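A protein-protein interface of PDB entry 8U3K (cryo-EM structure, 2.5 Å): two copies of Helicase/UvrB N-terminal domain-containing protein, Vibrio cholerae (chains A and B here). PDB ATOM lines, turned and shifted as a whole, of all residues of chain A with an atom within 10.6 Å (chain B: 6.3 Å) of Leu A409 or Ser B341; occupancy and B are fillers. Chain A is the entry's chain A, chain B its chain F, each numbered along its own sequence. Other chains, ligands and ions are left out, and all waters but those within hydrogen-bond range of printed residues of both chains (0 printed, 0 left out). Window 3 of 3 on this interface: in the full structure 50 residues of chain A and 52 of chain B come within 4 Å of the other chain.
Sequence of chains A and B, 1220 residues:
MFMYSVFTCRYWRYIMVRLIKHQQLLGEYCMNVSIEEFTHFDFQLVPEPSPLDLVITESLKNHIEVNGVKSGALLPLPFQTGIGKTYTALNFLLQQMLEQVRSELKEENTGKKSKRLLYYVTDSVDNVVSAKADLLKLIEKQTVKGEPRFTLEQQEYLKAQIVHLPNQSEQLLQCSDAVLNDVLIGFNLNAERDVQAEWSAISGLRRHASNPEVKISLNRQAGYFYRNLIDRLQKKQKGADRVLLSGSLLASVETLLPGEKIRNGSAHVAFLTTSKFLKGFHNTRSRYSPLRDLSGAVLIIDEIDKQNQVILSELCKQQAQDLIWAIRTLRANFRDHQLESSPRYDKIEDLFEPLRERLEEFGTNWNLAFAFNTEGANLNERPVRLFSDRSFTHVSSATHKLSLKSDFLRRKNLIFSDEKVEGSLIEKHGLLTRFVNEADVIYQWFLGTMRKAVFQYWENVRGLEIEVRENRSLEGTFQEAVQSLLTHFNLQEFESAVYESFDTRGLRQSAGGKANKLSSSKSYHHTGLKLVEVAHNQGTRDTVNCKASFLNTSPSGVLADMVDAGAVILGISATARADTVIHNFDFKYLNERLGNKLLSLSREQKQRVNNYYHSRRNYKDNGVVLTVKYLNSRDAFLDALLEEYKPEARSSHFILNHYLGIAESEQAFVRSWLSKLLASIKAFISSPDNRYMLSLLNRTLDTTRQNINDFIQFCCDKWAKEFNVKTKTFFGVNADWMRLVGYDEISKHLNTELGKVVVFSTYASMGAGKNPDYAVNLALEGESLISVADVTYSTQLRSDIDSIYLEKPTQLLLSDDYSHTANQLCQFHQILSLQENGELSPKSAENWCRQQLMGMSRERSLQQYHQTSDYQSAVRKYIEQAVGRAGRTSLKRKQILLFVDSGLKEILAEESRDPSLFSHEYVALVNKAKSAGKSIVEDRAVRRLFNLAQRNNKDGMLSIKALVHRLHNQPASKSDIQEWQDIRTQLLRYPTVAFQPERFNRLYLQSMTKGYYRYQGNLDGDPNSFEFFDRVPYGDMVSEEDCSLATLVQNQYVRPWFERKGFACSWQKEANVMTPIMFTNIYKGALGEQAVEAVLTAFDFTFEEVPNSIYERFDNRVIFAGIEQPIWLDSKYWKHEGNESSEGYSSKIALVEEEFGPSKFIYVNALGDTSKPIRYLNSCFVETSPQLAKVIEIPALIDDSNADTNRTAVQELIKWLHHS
A ring nitrogen (NE2) of His B488 lies within hydrogen-bond range of the side-chain carboxylate (OD1) of Asp A542. NH1 of Arg A410 lies within salt-bridge range of OE2 of Glu B340. N of Arg A411 sits at hydrogen-bond distance from O of Glu B340 (2.6 Å). The side-chain hydroxyl (OG1) of Thr A543 sits at hydrogen-bond distance from a ring nitrogen (NE2) of His B488, 3.3 Å away. The side-chain hydroxyl (OH) of Tyr B345 lies close to the side-chain carboxylate (OD2) of Asp A542 (3.5 Å). NE2 of His B488 lies close to NZ of Lys A412.
N of Leu A409 is in hydrogen-bond range of OD1 of Asp A407, at 3.0 Å. The side-chain carboxylate (OE2) of Glu A375 lies within salt-bridge range of the guanidinium group (NH2) of Arg A410, 3.4 Å away. OG1 of Thr A543 sits at hydrogen-bond distance from NZ of Lys A412, 3.4 Å away. The side-chain hydroxyl (OH) of Tyr B345 is in hydrogen-bond range of a ring nitrogen (NE2) of His B488 (3.3 Å). The backbone NH (N) of Asp A407 lies within hydrogen-bond range of the backbone carbonyl oxygen (O) of Lys A412, at 3.0 Å. OE1 of Glu B340 is in hydrogen-bond range of OG of Ser B342, 2.8 Å away.
Among the printed residues, merely in contact across the chains: Leu A409 with Ser B341, Arg A411 with Leu B339, Arg A411 with Ser B341 and Lys A412 with Glu B340.
Phe A408 touches none of the printed residues of chain B. Leu A409 touches one residue of chain B. Printed residues of chain B within 4 Å of Arg A410: Glu B340 (3.4 Å). Printed residues of chain B within 4 Å of Arg A411: Leu B339 (3.2 Å), Glu B340 (2.6 Å) and Ser B341 (3.6 Å). Of the printed residues of chain B, Thr A543 touches His B488 (3.3 Å). Of chain A, only Arg A411 (3.2 Å) comes within 4 Å of Leu B339. Ser B341 touches two residues of chain A. Ser B342 touches none of the printed residues of chain A. Pro B343 touches none of the printed residues of chain A. Printed residues of chain A within 4 Å of Tyr B345: Asp A542. Printed residues of chain A within 4 Å of His B488: Lys A412, Asp A542 and Thr A543. The nearest residue of chain A that does not touch Ser B341 is Arg A410 (4.2 Å). The nearest printed residue of chain B that does not touch Thr A543 is Tyr B345 (5.4 Å).
Hydrophobic or aromatic side chains of chain B within 4 Å of the printed part of chain A: Tyr B345 and His B488. Printed residues of chain A that touch a printed residue of chain B: Leu A409, Arg A410, Arg A411, Lys A412, Asp A542 and Thr A543. Among the printed residues, Asp or Glu carboxylates within 4 Å of a Lys or Arg side-chain nitrogen of the other chain: Arg A410 with Glu B340 (3.6 Å).
No position is printed for both chains.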
ATOM      1  N   ASN A 367     -15.653 -11.160 -33.862  1.00  0.00           N
ATOM      2  CA  ASN A 367     -16.485 -12.202 -33.262  1.00  0.00           C
ATOM      3  C   ASN A 367     -16.849 -11.862 -31.823  1.00  0.00           C
ATOM      4  O   ASN A 367     -16.430 -12.518 -30.873  1.00  0.00           O
ATOM      5  CB  ASN A 367     -15.810 -13.569 -33.342  1.00  0.00           C
ATOM      6  CG  ASN A 367     -15.711 -14.075 -34.749  1.00  0.00           C
ATOM      7  OD1 ASN A 367     -16.717 -14.269 -35.417  1.00  0.00           O
ATOM      8  ND2 ASN A 367     -14.495 -14.296 -35.212  1.00  0.00           N
ATOM      9  N   ALA A 369     -19.573 -12.267 -30.439  1.00  0.00           N
ATOM     10  CA  ALA A 369     -20.465 -13.229 -29.811  1.00  0.00           C
ATOM     11  C   ALA A 369     -19.753 -14.007 -28.720  1.00  0.00           C
ATOM     12  O   ALA A 369     -20.396 -14.531 -27.808  1.00  0.00           O
ATOM     13  CB  ALA A 369     -21.027 -14.184 -30.855  1.00  0.00           C
ATOM     14  N   PHE A 370     -18.433 -14.091 -28.793  1.00  0.00           N
ATOM     15  CA  PHE A 370     -17.633 -14.820 -27.826  1.00  0.00           C
ATOM     16  C   PHE A 370     -16.990 -13.846 -26.857  1.00  0.00           C
ATOM     17  O   PHE A 370     -16.766 -12.683 -27.191  1.00  0.00           O
ATOM     18  CB  PHE A 370     -16.542 -15.633 -28.515  1.00  0.00           C
ATOM     19  CG  PHE A 370     -17.029 -16.480 -29.646  1.00  0.00           C
ATOM     20  CD1 PHE A 370     -18.279 -17.058 -29.621  1.00  0.00           C
ATOM     21  CD2 PHE A 370     -16.220 -16.707 -30.736  1.00  0.00           C
ATOM     22  CE1 PHE A 370     -18.710 -17.829 -30.663  1.00  0.00           C
ATOM     23  CE2 PHE A 370     -16.649 -17.481 -31.773  1.00  0.00           C
ATOM     24  CZ  PHE A 370     -17.895 -18.042 -31.737  1.00  0.00           C
ATOM     25  N   ALA A 371     -16.696 -14.325 -25.658  1.00  0.00           N
ATOM     26  CA  ALA A 371     -15.910 -13.547 -24.722  1.00  0.00           C
ATOM     27  C   ALA A 371     -14.427 -13.750 -25.005  1.00  0.00           C
ATOM     28  O   ALA A 371     -14.037 -14.476 -25.918  1.00  0.00           O
ATOM     29  CB  ALA A 371     -16.252 -13.929 -23.287  1.00  0.00           C
ATOM     30  N   GLU A 375      -4.595 -17.183 -23.388  1.00  0.00           N
ATOM     31  CA  GLU A 375      -4.184 -18.561 -23.593  1.00  0.00           C
ATOM     32  C   GLU A 375      -2.668 -18.661 -23.555  1.00  0.00           C
ATOM     33  O   GLU A 375      -1.977 -17.877 -24.211  1.00  0.00           O
ATOM     34  CB  GLU A 375      -4.697 -19.084 -24.930  1.00  0.00           C
ATOM     35  CG  GLU A 375      -4.248 -20.488 -25.245  1.00  0.00           C
ATOM     36  CD  GLU A 375      -4.781 -20.978 -26.570  1.00  0.00           C
ATOM     37  OE1 GLU A 375      -4.258 -20.537 -27.615  1.00  0.00           O
ATOM     38  OE2 GLU A 375      -5.720 -21.801 -26.569  1.00  0.00           O
ATOM     39  N   LYS A 405      -7.178 -14.549 -31.655  1.00  0.00           N
ATOM     40  CA  LYS A 405      -7.669 -15.654 -32.465  1.00  0.00           C
ATOM     41  C   LYS A 405      -9.052 -16.060 -31.982  1.00  0.00           C
ATOM     42  O   LYS A 405      -9.289 -16.141 -30.775  1.00  0.00           O
ATOM     43  CB  LYS A 405      -6.702 -16.830 -32.372  1.00  0.00           C
ATOM     44  CG  LYS A 405      -7.241 -18.147 -32.835  1.00  0.00           C
ATOM     45  CD  LYS A 405      -6.729 -19.261 -31.945  1.00  0.00           C
ATOM     46  CE  LYS A 405      -5.221 -19.251 -31.848  1.00  0.00           C
ATOM     47  NZ  LYS A 405      -4.717 -20.279 -30.900  1.00  0.00           N
ATOM     48  N   SER A 406      -9.961 -16.311 -32.918  1.00  0.00           N
ATOM     49  CA  SER A 406     -11.304 -16.777 -32.589  1.00  0.00           C
ATOM     50  C   SER A 406     -11.368 -18.283 -32.789  1.00  0.00           C
ATOM     51  O   SER A 406     -11.218 -18.773 -33.911  1.00  0.00           O
ATOM     52  CB  SER A 406     -12.346 -16.079 -33.452  1.00  0.00           C
ATOM     53  OG  SER A 406     -12.329 -14.683 -33.239  1.00  0.00           O
ATOM     54  N   ASP A 407     -11.599 -19.018 -31.708  1.00  0.00           N
ATOM     55  CA  ASP A 407     -11.717 -20.467 -31.760  1.00  0.00           C
ATOM     56  C   ASP A 407     -13.192 -20.831 -31.780  1.00  0.00           C
ATOM     57  O   ASP A 407     -13.886 -20.665 -30.775  1.00  0.00           O
ATOM     58  CB  ASP A 407     -11.022 -21.112 -30.565  1.00  0.00           C
ATOM     59  CG  ASP A 407     -10.886 -22.618 -30.707  1.00  0.00           C
ATOM     60  OD1 ASP A 407     -11.473 -23.203 -31.639  1.00  0.00           O
ATOM     61  OD2 ASP A 407     -10.173 -23.223 -29.886  1.00  0.00           O
ATOM     62  N   PHE A 408     -13.664 -21.335 -32.914  1.00  0.00           N
ATOM     63  CA  PHE A 408     -15.055 -21.725 -33.066  1.00  0.00           C
ATOM     64  C   PHE A 408     -15.342 -23.118 -32.535  1.00  0.00           C
ATOM     65  O   PHE A 408     -16.511 -23.461 -32.350  1.00  0.00           O
ATOM     66  CB  PHE A 408     -15.468 -21.646 -34.532  1.00  0.00           C
ATOM     67  CG  PHE A 408     -15.509 -20.256 -35.068  1.00  0.00           C
ATOM     68  CD1 PHE A 408     -14.394 -19.694 -35.649  1.00  0.00           C
ATOM     69  CD2 PHE A 408     -16.663 -19.509 -34.989  1.00  0.00           C
ATOM     70  CE1 PHE A 408     -14.432 -18.414 -36.143  1.00  0.00           C
ATOM     71  CE2 PHE A 408     -16.705 -18.230 -35.482  1.00  0.00           C
ATOM     72  CZ  PHE A 408     -15.589 -17.682 -36.059  1.00  0.00           C
ATOM     73  N   LEU A 409     -14.314 -23.928 -32.287  1.00  0.00           N
ATOM     74  CA  LEU A 409     -14.533 -25.203 -31.615  1.00  0.00           C
ATOM     75  C   LEU A 409     -14.972 -24.970 -30.175  1.00  0.00           C
ATOM     76  O   LEU A 409     -15.979 -25.524 -29.728  1.00  0.00           O
ATOM     77  CB  LEU A 409     -13.262 -26.052 -31.685  1.00  0.00           C
ATOM     78  CG  LEU A 409     -13.241 -27.487 -31.150  1.00  0.00           C
ATOM     79  CD1 LEU A 409     -12.820 -27.558 -29.683  1.00  0.00           C
ATOM     80  CD2 LEU A 409     -14.580 -28.176 -31.372  1.00  0.00           C
ATOM     81  N   ARG A 410     -14.235 -24.144 -29.446  1.00  0.00           N
ATOM     82  CA  ARG A 410     -14.759 -23.532 -28.235  1.00  0.00           C
ATOM     83  C   ARG A 410     -15.627 -22.360 -28.668  1.00  0.00           C
ATOM     84  O   ARG A 410     -15.983 -22.212 -29.835  1.00  0.00           O
ATOM     85  CB  ARG A 410     -13.632 -23.095 -27.313  1.00  0.00           C
ATOM     86  CG  ARG A 410     -12.577 -24.142 -27.096  1.00  0.00           C
ATOM     87  CD  ARG A 410     -11.222 -23.509 -26.880  1.00  0.00           C
ATOM     88  NE  ARG A 410     -11.055 -23.007 -25.524  1.00  0.00           N
ATOM     89  CZ  ARG A 410      -9.876 -22.739 -24.974  1.00  0.00           C
ATOM     90  NH1 ARG A 410      -9.807 -22.282 -23.735  1.00  0.00           N
ATOM     91  NH2 ARG A 410      -8.765 -22.928 -25.669  1.00  0.00           N
ATOM     92  N   ARG A 411     -15.999 -21.512 -27.743  1.00  0.00           N
ATOM     93  CA  ARG A 411     -16.609 -20.247 -28.122  1.00  0.00           C
ATOM     94  C   ARG A 411     -15.852 -19.185 -27.350  1.00  0.00           C
ATOM     95  O   ARG A 411     -16.303 -18.706 -26.310  1.00  0.00           O
ATOM     96  CB  ARG A 411     -18.091 -20.239 -27.839  1.00  0.00           C
ATOM     97  CG  ARG A 411     -18.935 -20.876 -28.926  1.00  0.00           C
ATOM     98  CD  ARG A 411     -19.057 -22.362 -28.754  1.00  0.00           C
ATOM     99  NE  ARG A 411     -20.246 -22.890 -29.408  1.00  0.00           N
ATOM    100  CZ  ARG A 411     -21.411 -23.067 -28.801  1.00  0.00           C
ATOM    101  NH1 ARG A 411     -22.441 -23.553 -29.476  1.00  0.00           N
ATOM    102  NH2 ARG A 411     -21.547 -22.767 -27.519  1.00  0.00           N
ATOM    103  N   LYS A 412     -14.702 -18.799 -27.884  1.00  0.00           N
ATOM    104  CA  LYS A 412     -13.781 -17.930 -27.181  1.00  0.00           C
ATOM    105  C   LYS A 412     -12.912 -17.198 -28.181  1.00  0.00           C
ATOM    106  O   LYS A 412     -12.561 -17.732 -29.231  1.00  0.00           O
ATOM    107  CB  LYS A 412     -12.875 -18.709 -26.235  1.00  0.00           C
ATOM    108  CG  LYS A 412     -13.432 -18.897 -24.867  1.00  0.00           C
ATOM    109  CD  LYS A 412     -13.539 -17.606 -24.123  1.00  0.00           C
ATOM    110  CE  LYS A 412     -13.565 -17.888 -22.653  1.00  0.00           C
ATOM    111  NZ  LYS A 412     -13.871 -16.693 -21.865  1.00  0.00           N
ATOM    112  N   ASN A 413     -12.567 -15.973 -27.834  1.00  0.00           N
ATOM    113  CA  ASN A 413     -11.521 -15.234 -28.513  1.00  0.00           C
ATOM    114  C   ASN A 413     -10.295 -15.287 -27.623  1.00  0.00           C
ATOM    115  O   ASN A 413     -10.347 -14.860 -26.468  1.00  0.00           O
ATOM    116  CB  ASN A 413     -11.960 -13.802 -28.777  1.00  0.00           C
ATOM    117  CG  ASN A 413     -13.117 -13.728 -29.719  1.00  0.00           C
ATOM    118  OD1 ASN A 413     -13.102 -14.347 -30.772  1.00  0.00           O
ATOM    119  ND2 ASN A 413     -14.135 -12.982 -29.348  1.00  0.00           N
ATOM    120  N   LEU A 414      -9.204 -15.825 -28.145  1.00  0.00           N
ATOM    121  CA  LEU A 414      -8.051 -16.165 -27.328  1.00  0.00           C
ATOM    122  C   LEU A 414      -6.914 -15.204 -27.625  1.00  0.00           C
ATOM    123  O   LEU A 414      -6.522 -15.038 -28.783  1.00  0.00           O
ATOM    124  CB  LEU A 414      -7.627 -17.608 -27.576  1.00  0.00           C
ATOM    125  CG  LEU A 414      -8.706 -18.603 -27.172  1.00  0.00           C
ATOM    126  CD1 LEU A 414      -8.394 -19.971 -27.711  1.00  0.00           C
ATOM    127  CD2 LEU A 414      -8.833 -18.640 -25.673  1.00  0.00           C
ATOM    128  N   ASP A 542     -11.472 -17.280 -16.450  1.00  0.00           N
ATOM    129  CA  ASP A 542     -11.615 -17.624 -17.849  1.00  0.00           C
ATOM    130  C   ASP A 542     -12.180 -16.497 -18.693  1.00  0.00           C
ATOM    131  O   ASP A 542     -12.578 -16.746 -19.832  1.00  0.00           O
ATOM    132  CB  ASP A 542     -12.493 -18.871 -18.011  1.00  0.00           C
ATOM    133  CG  ASP A 542     -13.866 -18.692 -17.424  1.00  0.00           C
ATOM    134  OD1 ASP A 542     -14.855 -18.914 -18.149  1.00  0.00           O
ATOM    135  OD2 ASP A 542     -13.962 -18.329 -16.236  1.00  0.00           O
ATOM    136  N   THR A 543     -12.236 -15.274 -18.179  1.00  0.00           N
ATOM    137  CA  THR A 543     -12.634 -14.143 -18.995  1.00  0.00           C
ATOM    138  C   THR A 543     -11.714 -12.981 -18.656  1.00  0.00           C
ATOM    139  O   THR A 543     -11.250 -12.853 -17.523  1.00  0.00           O
ATOM    140  CB  THR A 543     -14.110 -13.785 -18.779  1.00  0.00           C
ATOM    141  OG1 THR A 543     -14.919 -14.892 -19.178  1.00  0.00           O
ATOM    142  CG2 THR A 543     -14.515 -12.632 -19.658  1.00  0.00           C
ATOM    143  N   LEU B 339     -21.494 -18.930 -24.209  1.00  0.00           N
ATOM    144  CA  LEU B 339     -20.415 -19.258 -23.296  1.00  0.00           C
ATOM    145  C   LEU B 339     -19.417 -20.228 -23.926  1.00  0.00           C
ATOM    146  O   LEU B 339     -19.574 -20.672 -25.062  1.00  0.00           O
ATOM    147  CB  LEU B 339     -20.967 -19.813 -21.983  1.00  0.00           C
ATOM    148  CG  LEU B 339     -22.091 -20.839 -21.994  1.00  0.00           C
ATOM    149  CD1 LEU B 339     -21.549 -22.249 -22.137  1.00  0.00           C
ATOM    150  CD2 LEU B 339     -22.865 -20.707 -20.713  1.00  0.00           C
ATOM    151  N   GLU B 340     -18.404 -20.584 -23.133  1.00  0.00           N
ATOM    152  CA  GLU B 340     -17.116 -21.025 -23.662  1.00  0.00           C
ATOM    153  C   GLU B 340     -17.190 -22.339 -24.429  1.00  0.00           C
ATOM    154  O   GLU B 340     -16.413 -22.538 -25.371  1.00  0.00           O
ATOM    155  CB  GLU B 340     -16.113 -21.138 -22.519  1.00  0.00           C
ATOM    156  CG  GLU B 340     -14.751 -21.669 -22.912  1.00  0.00           C
ATOM    157  CD  GLU B 340     -13.739 -21.557 -21.799  1.00  0.00           C
ATOM    158  OE1 GLU B 340     -14.002 -22.088 -20.701  1.00  0.00           O
ATOM    159  OE2 GLU B 340     -12.673 -20.952 -22.022  1.00  0.00           O
ATOM    160  N   SER B 341     -18.112 -23.232 -24.064  1.00  0.00           N
ATOM    161  CA  SER B 341     -18.141 -24.615 -24.555  1.00  0.00           C
ATOM    162  C   SER B 341     -16.867 -25.361 -24.161  1.00  0.00           C
ATOM    163  O   SER B 341     -16.096 -25.831 -24.993  1.00  0.00           O
ATOM    164  CB  SER B 341     -18.371 -24.692 -26.065  1.00  0.00           C
ATOM    165  OG  SER B 341     -18.244 -26.025 -26.514  1.00  0.00           O
ATOM    166  N   SER B 342     -16.677 -25.464 -22.856  1.00  0.00           N
ATOM    167  CA  SER B 342     -15.579 -26.166 -22.217  1.00  0.00           C
ATOM    168  C   SER B 342     -16.190 -27.084 -21.172  1.00  0.00           C
ATOM    169  O   SER B 342     -17.370 -26.940 -20.837  1.00  0.00           O
ATOM    170  CB  SER B 342     -14.595 -25.177 -21.582  1.00  0.00           C
ATOM    171  OG  SER B 342     -15.120 -24.631 -20.391  1.00  0.00           O
ATOM    172  N   PRO B 343     -15.431 -28.060 -20.663  1.00  0.00           N
ATOM    173  CA  PRO B 343     -16.012 -28.992 -19.683  1.00  0.00           C
ATOM    174  C   PRO B 343     -16.539 -28.339 -18.419  1.00  0.00           C
ATOM    175  O   PRO B 343     -17.411 -28.921 -17.765  1.00  0.00           O
ATOM    176  CB  PRO B 343     -14.847 -29.941 -19.371  1.00  0.00           C
ATOM    177  CG  PRO B 343     -13.641 -29.289 -19.929  1.00  0.00           C
ATOM    178  CD  PRO B 343     -14.119 -28.544 -21.116  1.00  0.00           C
ATOM    179  N   TYR B 345     -18.346 -25.761 -18.369  1.00  0.00           N
ATOM    180  CA  TYR B 345     -19.646 -25.211 -18.726  1.00  0.00           C
ATOM    181  C   TYR B 345     -20.575 -26.255 -19.319  1.00  0.00           C
ATOM    182  O   TYR B 345     -21.387 -25.923 -20.183  1.00  0.00           O
ATOM    183  CB  TYR B 345     -19.485 -24.055 -19.711  1.00  0.00           C
ATOM    184  CG  TYR B 345     -18.803 -22.852 -19.125  1.00  0.00           C
ATOM    185  CD1 TYR B 345     -19.448 -22.052 -18.206  1.00  0.00           C
ATOM    186  CD2 TYR B 345     -17.514 -22.521 -19.487  1.00  0.00           C
ATOM    187  CE1 TYR B 345     -18.830 -20.963 -17.662  1.00  0.00           C
ATOM    188  CE2 TYR B 345     -16.888 -21.434 -18.946  1.00  0.00           C
ATOM    189  CZ  TYR B 345     -17.551 -20.660 -18.034  1.00  0.00           C
ATOM    190  OH  TYR B 345     -16.936 -19.564 -17.489  1.00  0.00           O
ATOM    191  N   GLU B 349     -25.616 -24.181 -21.205  1.00  0.00           N
ATOM    192  CA  GLU B 349     -26.297 -23.486 -22.293  1.00  0.00           C
ATOM    193  C   GLU B 349     -27.662 -24.098 -22.565  1.00  0.00           C
ATOM    194  O   GLU B 349     -28.586 -23.409 -23.015  1.00  0.00           O
ATOM    195  CB  GLU B 349     -25.440 -23.502 -23.556  1.00  0.00           C
ATOM    196  CG  GLU B 349     -24.858 -24.856 -23.916  1.00  0.00           C
ATOM    197  CD  GLU B 349     -23.551 -25.155 -23.197  1.00  0.00           C
ATOM    198  OE1 GLU B 349     -22.476 -25.015 -23.819  1.00  0.00           O
ATOM    199  OE2 GLU B 349     -23.602 -25.528 -22.007  1.00  0.00           O
ATOM    200  N   HIS B 488     -19.727 -13.864 -19.344  1.00  0.00           N
ATOM    201  CA  HIS B 488     -19.823 -14.509 -20.644  1.00  0.00           C
ATOM    202  C   HIS B 488     -21.015 -14.023 -21.443  1.00  0.00           C
ATOM    203  O   HIS B 488     -20.942 -13.984 -22.672  1.00  0.00           O
ATOM    204  CB  HIS B 488     -19.911 -16.017 -20.483  1.00  0.00           C
ATOM    205  CG  HIS B 488     -18.585 -16.696 -20.492  1.00  0.00           C
ATOM    206  ND1 HIS B 488     -18.089 -17.335 -21.603  1.00  0.00           N
ATOM    207  CD2 HIS B 488     -17.654 -16.844 -19.523  1.00  0.00           C
ATOM    208  CE1 HIS B 488     -16.905 -17.842 -21.321  1.00  0.00           C
ATOM    209  NE2 HIS B 488     -16.619 -17.558 -20.066  1.00  0.00           N
